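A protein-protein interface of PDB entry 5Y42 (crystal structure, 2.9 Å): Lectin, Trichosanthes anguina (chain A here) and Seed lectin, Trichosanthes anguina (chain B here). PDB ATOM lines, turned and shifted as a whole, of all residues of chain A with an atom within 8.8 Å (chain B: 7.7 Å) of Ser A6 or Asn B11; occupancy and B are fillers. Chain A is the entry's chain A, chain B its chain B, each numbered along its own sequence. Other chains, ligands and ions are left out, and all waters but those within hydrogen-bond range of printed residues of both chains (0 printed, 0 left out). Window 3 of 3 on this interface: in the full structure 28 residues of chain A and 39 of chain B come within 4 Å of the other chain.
O of Leu A3 sits at hydrogen-bond distance from N of Thr B9.
O of Thr B9 is in hydrogen-bond range of N of Leu A5 (3.1 Å).
The backbone carbonyl oxygen of Leu A5 sits close to the side-chain amide oxygen of Asn B11 (3.5 Å).
N of Ser A6 sits close to OD1 of Asn B11.
The backbone NH (N) of Asn B11 sits at hydrogen-bond distance from the side-chain carboxylate (OD1) of Asp B89 (2.8 Å).
O of Asp B89 is in hydrogen-bond range of OG of Ser B93, at 3.4 Å.
Among the printed residues, pairs that only touch across the chains: Arg A4 with Thr B9 (3.8 Å), Leu A5 with Val B85 (3.9 Å) and Leu A5 with Asp B89 (3.6 Å).
Of the printed residues of chain B, Arg A4 touches Thr B9 (3.8 Å).
Of chain B, only Asn B11 comes within 4 Å of Ser A6.
No residue of chain A comes within 4 Å of Ser B10.
Asn B11 touches just these residues of chain A: Leu A5 (3.5 Å) and Ser A6 (3.4 Å).
Printed residues of chain A within 4 Å of Asp B89: Leu A5.
Of the 13 printed residues of chain B, 4 touch a printed residue of chain A.
Of the 8 printed residues of chain A, 4 touch a printed residue of chain B.
Hydrophobic or aromatic side chains of chain A within 4 Å of the printed part of chain B: Leu A5.
Among the printed residues, no Asp or Glu carboxylate lies within 4 Å of a Lys or Arg side-chain nitrogen of the other chain.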
ATOM      1  N   LEU A   3      -1.282 -21.998 -22.238  1.00  0.00           N
ATOM      2  CA  LEU A   3      -2.161 -20.843 -22.320  1.00  0.00           C
ATOM      3  C   LEU A   3      -2.956 -21.009 -23.612  1.00  0.00           C
ATOM      4  O   LEU A   3      -2.434 -20.975 -24.707  1.00  0.00           O
ATOM      5  CB  LEU A   3      -1.431 -19.504 -22.304  1.00  0.00           C
ATOM      6  CG  LEU A   3      -2.306 -18.239 -22.337  1.00  0.00           C
ATOM      7  CD1 LEU A   3      -3.252 -18.195 -21.150  1.00  0.00           C
ATOM      8  CD2 LEU A   3      -1.477 -16.964 -22.380  1.00  0.00           C
ATOM      9  N   ARG A   4      -4.272 -21.128 -23.452  1.00  0.00           N
ATOM     10  CA  ARG A   4      -5.243 -21.125 -24.534  1.00  0.00           C
ATOM     11  C   ARG A   4      -5.870 -19.740 -24.595  1.00  0.00           C
ATOM     12  O   ARG A   4      -6.412 -19.205 -23.612  1.00  0.00           O
ATOM     13  CB  ARG A   4      -6.324 -22.174 -24.315  1.00  0.00           C
ATOM     14  CG  ARG A   4      -5.851 -23.575 -24.653  1.00  0.00           C
ATOM     15  CD  ARG A   4      -6.995 -24.592 -24.652  1.00  0.00           C
ATOM     16  NE  ARG A   4      -6.510 -25.982 -24.769  1.00  0.00           N
ATOM     17  CZ  ARG A   4      -5.920 -26.702 -23.798  1.00  0.00           C
ATOM     18  NH1 ARG A   4      -5.705 -26.198 -22.580  1.00  0.00           N
ATOM     19  NH2 ARG A   4      -5.521 -27.953 -24.047  1.00  0.00           N
ATOM     20  N   LEU A   5      -5.911 -19.199 -25.784  1.00  0.00           N
ATOM     21  CA  LEU A   5      -6.506 -17.892 -26.026  1.00  0.00           C
ATOM     22  C   LEU A   5      -8.014 -17.912 -26.315  1.00  0.00           C
ATOM     23  O   LEU A   5      -8.570 -16.843 -26.308  1.00  0.00           O
ATOM     24  CB  LEU A   5      -5.802 -17.179 -27.171  1.00  0.00           C
ATOM     25  CG  LEU A   5      -4.420 -16.590 -26.915  1.00  0.00           C
ATOM     26  CD1 LEU A   5      -4.215 -15.457 -27.916  1.00  0.00           C
ATOM     27  CD2 LEU A   5      -4.201 -16.073 -25.500  1.00  0.00           C
ATOM     28  N   SER A   6      -8.605 -19.055 -26.676  1.00  0.00           N
ATOM     29  CA  SER A   6     -10.066 -19.147 -26.851  1.00  0.00           C
ATOM     30  C   SER A   6     -10.738 -19.109 -25.477  1.00  0.00           C
ATOM     31  O   SER A   6     -11.775 -18.461 -25.322  1.00  0.00           O
ATOM     32  CB  SER A   6     -10.444 -20.408 -27.624  1.00  0.00           C
ATOM     33  OG  SER A   6      -9.892 -21.545 -26.996  1.00  0.00           O
ATOM     34  N   GLU A   7     -10.119 -19.781 -24.499  1.00  0.00           N
ATOM     35  CA  GLU A   7     -10.647 -19.867 -23.109  1.00  0.00           C
ATOM     36  C   GLU A   7     -10.046 -18.742 -22.217  1.00  0.00           C
ATOM     37  O   GLU A   7      -9.603 -19.029 -21.091  1.00  0.00           O
ATOM     38  CB  GLU A   7     -10.340 -21.272 -22.475  1.00  0.00           C
ATOM     39  CG  GLU A   7     -10.675 -22.519 -23.330  1.00  0.00           C
ATOM     40  CD  GLU A   7     -10.556 -23.870 -22.598  1.00  0.00           C
ATOM     41  OE1 GLU A   7     -10.680 -23.920 -21.348  1.00  0.00           O
ATOM     42  OE2 GLU A   7     -10.368 -24.903 -23.289  1.00  0.00           O
ATOM     43  N   ALA A   8      -9.911 -17.546 -22.740  1.00  0.00           N
ATOM     44  CA  ALA A   8      -9.042 -16.539 -22.129  1.00  0.00           C
ATOM     45  C   ALA A   8      -9.692 -15.287 -21.658  1.00  0.00           C
ATOM     46  O   ALA A   8     -10.276 -14.590 -22.446  1.00  0.00           O
ATOM     47  CB  ALA A   8      -7.944 -16.200 -23.113  1.00  0.00           C
ATOM     48  N   ASN A   9      -9.591 -15.014 -20.356  1.00  0.00           N
ATOM     49  CA  ASN A   9      -9.934 -13.730 -19.759  1.00  0.00           C
ATOM     50  C   ASN A   9      -8.785 -13.302 -18.847  1.00  0.00           C
ATOM     51  O   ASN A   9      -7.795 -14.039 -18.646  1.00  0.00           O
ATOM     52  CB  ASN A   9     -11.289 -13.811 -19.002  1.00  0.00           C
ATOM     53  CG  ASN A   9     -11.291 -14.815 -17.830  1.00  0.00           C
ATOM     54  OD1 ASN A   9     -10.365 -15.636 -17.637  1.00  0.00           O
ATOM     55  ND2 ASN A   9     -12.351 -14.744 -17.032  1.00  0.00           N
ATOM     56  N   THR A  12      -7.793 -16.050 -16.263  1.00  0.00           N
ATOM     57  CA  THR A  12      -7.000 -17.189 -16.719  1.00  0.00           C
ATOM     58  C   THR A  12      -5.571 -16.741 -17.092  1.00  0.00           C
ATOM     59  O   THR A  12      -4.621 -17.476 -16.884  1.00  0.00           O
ATOM     60  CB  THR A  12      -7.677 -17.942 -17.890  1.00  0.00           C
ATOM     61  OG1 THR A  12      -7.952 -17.024 -18.941  1.00  0.00           O
ATOM     62  CG2 THR A  12      -8.986 -18.585 -17.443  1.00  0.00           C
ATOM     63  N   THR B   9      -1.361 -21.503 -27.125  1.00  0.00           N
ATOM     64  CA  THR B   9      -2.291 -21.937 -28.177  1.00  0.00           C
ATOM     65  C   THR B   9      -3.162 -20.796 -28.672  1.00  0.00           C
ATOM     66  O   THR B   9      -3.825 -20.128 -27.890  1.00  0.00           O
ATOM     67  CB  THR B   9      -3.236 -23.071 -27.717  1.00  0.00           C
ATOM     68  OG1 THR B   9      -2.457 -24.102 -27.105  1.00  0.00           O
ATOM     69  CG2 THR B   9      -4.056 -23.686 -28.909  1.00  0.00           C
ATOM     70  N   SER B  10      -3.158 -20.603 -29.989  1.00  0.00           N
ATOM     71  CA  SER B  10      -3.913 -19.505 -30.623  1.00  0.00           C
ATOM     72  C   SER B  10      -5.422 -19.763 -30.671  1.00  0.00           C
ATOM     73  O   SER B  10      -5.903 -20.868 -30.384  1.00  0.00           O
ATOM     74  CB  SER B  10      -3.387 -19.226 -32.012  1.00  0.00           C
ATOM     75  OG  SER B  10      -3.691 -20.306 -32.838  1.00  0.00           O
ATOM     76  N   ASN B  11      -6.161 -18.754 -31.053  1.00  0.00           N
ATOM     77  CA  ASN B  11      -7.603 -18.923 -31.426  1.00  0.00           C
ATOM     78  C   ASN B  11      -7.875 -19.857 -32.584  1.00  0.00           C
ATOM     79  O   ASN B  11      -8.997 -20.391 -32.641  1.00  0.00           O
ATOM     80  CB  ASN B  11      -8.247 -17.577 -31.777  1.00  0.00           C
ATOM     81  CG  ASN B  11      -8.751 -16.840 -30.564  1.00  0.00           C
ATOM     82  OD1 ASN B  11      -9.338 -17.442 -29.655  1.00  0.00           O
ATOM     83  ND2 ASN B  11      -8.536 -15.530 -30.549  1.00  0.00           N
ATOM     84  N   GLN B  12      -6.907 -20.031 -33.496  1.00  0.00           N
ATOM     85  CA  GLN B  12      -7.057 -21.023 -34.581  1.00  0.00           C
ATOM     86  C   GLN B  12      -6.632 -22.426 -34.137  1.00  0.00           C
ATOM     87  O   GLN B  12      -6.596 -23.343 -34.947  1.00  0.00           O
ATOM     88  CB  GLN B  12      -6.304 -20.569 -35.827  1.00  0.00           C
ATOM     89  CG  GLN B  12      -6.523 -19.084 -36.133  1.00  0.00           C
ATOM     90  CD  GLN B  12      -6.122 -18.657 -37.550  1.00  0.00           C
ATOM     91  OE1 GLN B  12      -5.135 -19.121 -38.083  1.00  0.00           O
ATOM     92  NE2 GLN B  12      -6.878 -17.738 -38.148  1.00  0.00           N
ATOM     93  N   ASP B  13      -6.407 -22.609 -32.847  1.00  0.00           N
ATOM     94  CA  ASP B  13      -5.952 -23.886 -32.249  1.00  0.00           C
ATOM     95  C   ASP B  13      -4.566 -24.323 -32.754  1.00  0.00           C
ATOM     96  O   ASP B  13      -4.298 -25.510 -32.877  1.00  0.00           O
ATOM     97  CB  ASP B  13      -7.027 -24.956 -32.497  1.00  0.00           C
ATOM     98  CG  ASP B  13      -7.157 -25.945 -31.357  1.00  0.00           C
ATOM     99  OD1 ASP B  13      -6.129 -26.287 -30.722  1.00  0.00           O
ATOM    100  OD2 ASP B  13      -8.303 -26.392 -31.112  1.00  0.00           O
ATOM    101  N   GLU B  14      -3.757 -23.375 -33.176  1.00  0.00           N
ATOM    102  CA  GLU B  14      -2.386 -23.702 -33.566  1.00  0.00           C
ATOM    103  C   GLU B  14      -1.566 -23.479 -32.272  1.00  0.00           C
ATOM    104  O   GLU B  14      -1.601 -22.359 -31.684  1.00  0.00           O
ATOM    105  CB  GLU B  14      -1.915 -22.907 -34.819  1.00  0.00           C
ATOM    106  CG  GLU B  14      -2.360 -21.457 -34.963  1.00  0.00           C
ATOM    107  CD  GLU B  14      -2.284 -20.896 -36.372  1.00  0.00           C
ATOM    108  OE1 GLU B  14      -2.042 -21.631 -37.357  1.00  0.00           O
ATOM    109  OE2 GLU B  14      -2.512 -19.683 -36.501  1.00  0.00           O
ATOM    110  N   VAL B  85      -4.482  -8.858 -26.466  1.00  0.00           N
ATOM    111  CA  VAL B  85      -5.023 -10.171 -26.820  1.00  0.00           C
ATOM    112  C   VAL B  85      -4.821 -10.530 -28.283  1.00  0.00           C
ATOM    113  O   VAL B  85      -4.322 -11.606 -28.576  1.00  0.00           O
ATOM    114  CB  VAL B  85      -6.502 -10.326 -26.417  1.00  0.00           C
ATOM    115  CG1 VAL B  85      -6.998 -11.761 -26.649  1.00  0.00           C
ATOM    116  CG2 VAL B  85      -6.651  -9.995 -24.964  1.00  0.00           C
ATOM    117  N   ASP B  86      -5.209  -9.633 -29.200  1.00  0.00           N
ATOM    118  CA  ASP B  86      -5.067  -9.858 -30.610  1.00  0.00           C
ATOM    119  C   ASP B  86      -3.626  -9.835 -31.074  1.00  0.00           C
ATOM    120  O   ASP B  86      -3.242 -10.620 -31.930  1.00  0.00           O
ATOM    121  CB  ASP B  86      -5.900  -8.834 -31.433  1.00  0.00           C
ATOM    122  CG  ASP B  86      -7.397  -9.187 -31.504  1.00  0.00           C
ATOM    123  OD1 ASP B  86      -7.784 -10.306 -31.071  1.00  0.00           O
ATOM    124  OD2 ASP B  86      -8.180  -8.329 -31.991  1.00  0.00           O
ATOM    125  N   LEU B  88      -1.087 -10.924 -29.273  1.00  0.00           N
ATOM    126  CA  LEU B  88      -0.600 -12.214 -28.836  1.00  0.00           C
ATOM    127  C   LEU B  88      -1.064 -13.320 -29.770  1.00  0.00           C
ATOM    128  O   LEU B  88      -0.279 -14.206 -30.087  1.00  0.00           O
ATOM    129  CB  LEU B  88      -1.031 -12.465 -27.379  1.00  0.00           C
ATOM    130  CG  LEU B  88      -0.487 -13.726 -26.707  1.00  0.00           C
ATOM    131  CD1 LEU B  88       1.018 -13.786 -26.868  1.00  0.00           C
ATOM    132  CD2 LEU B  88      -0.864 -13.761 -25.236  1.00  0.00           C
ATOM    133  N   ASP B  89      -2.329 -13.268 -30.201  1.00  0.00           N
ATOM    134  CA  ASP B  89      -2.901 -14.269 -31.091  1.00  0.00           C
ATOM    135  C   ASP B  89      -2.134 -14.271 -32.429  1.00  0.00           C
ATOM    136  O   ASP B  89      -1.738 -15.361 -32.880  1.00  0.00           O
ATOM    137  CB  ASP B  89      -4.391 -13.933 -31.315  1.00  0.00           C
ATOM    138  CG  ASP B  89      -5.213 -15.133 -31.845  1.00  0.00           C
ATOM    139  OD1 ASP B  89      -4.865 -16.311 -31.603  1.00  0.00           O
ATOM    140  OD2 ASP B  89      -6.256 -14.899 -32.496  1.00  0.00           O
ATOM    141  N   PHE B  90      -1.960 -13.058 -32.999  1.00  0.00           N
ATOM    142  CA  PHE B  90      -1.200 -12.867 -34.187  1.00  0.00           C
ATOM    143  C   PHE B  90       0.224 -13.384 -34.044  1.00  0.00           C
ATOM    144  O   PHE B  90       0.742 -14.038 -34.947  1.00  0.00           O
ATOM    145  CB  PHE B  90      -1.107 -11.456 -34.812  1.00  0.00           C
ATOM    146  CG  PHE B  90      -2.423 -10.817 -35.125  1.00  0.00           C
ATOM    147  CD1 PHE B  90      -3.540 -11.572 -35.534  1.00  0.00           C
ATOM    148  CD2 PHE B  90      -2.550  -9.425 -35.019  1.00  0.00           C
ATOM    149  CE1 PHE B  90      -4.749 -10.944 -35.802  1.00  0.00           C
ATOM    150  CE2 PHE B  90      -3.757  -8.798 -35.287  1.00  0.00           C
ATOM    151  CZ  PHE B  90      -4.856  -9.557 -35.686  1.00  0.00           C
ATOM    152  N   ILE B  92       1.452 -15.675 -31.875  1.00  0.00           N
ATOM    153  CA  ILE B  92       1.510 -17.150 -31.771  1.00  0.00           C
ATOM    154  C   ILE B  92       1.385 -17.763 -33.153  1.00  0.00           C
ATOM    155  O   ILE B  92       2.217 -18.602 -33.556  1.00  0.00           O
ATOM    156  CB  ILE B  92       0.463 -17.764 -30.807  1.00  0.00           C
ATOM    157  CG1 ILE B  92       0.753 -17.323 -29.373  1.00  0.00           C
ATOM    158  CG2 ILE B  92       0.482 -19.308 -30.869  1.00  0.00           C
ATOM    159  CD1 ILE B  92      -0.409 -17.493 -28.414  1.00  0.00           C
ATOM    160  N   SER B  93       0.411 -17.233 -33.927  1.00  0.00           N
ATOM    161  CA  SER B  93       0.186 -17.670 -35.319  1.00  0.00           C
ATOM    162  C   SER B  93       1.427 -17.588 -36.192  1.00  0.00           C
ATOM    163  O   SER B  93       1.721 -18.527 -36.924  1.00  0.00           O
ATOM    164  CB  SER B  93      -1.067 -16.995 -35.941  1.00  0.00           C
ATOM    165  OG  SER B  93      -2.291 -17.539 -35.406  1.00  0.00           O
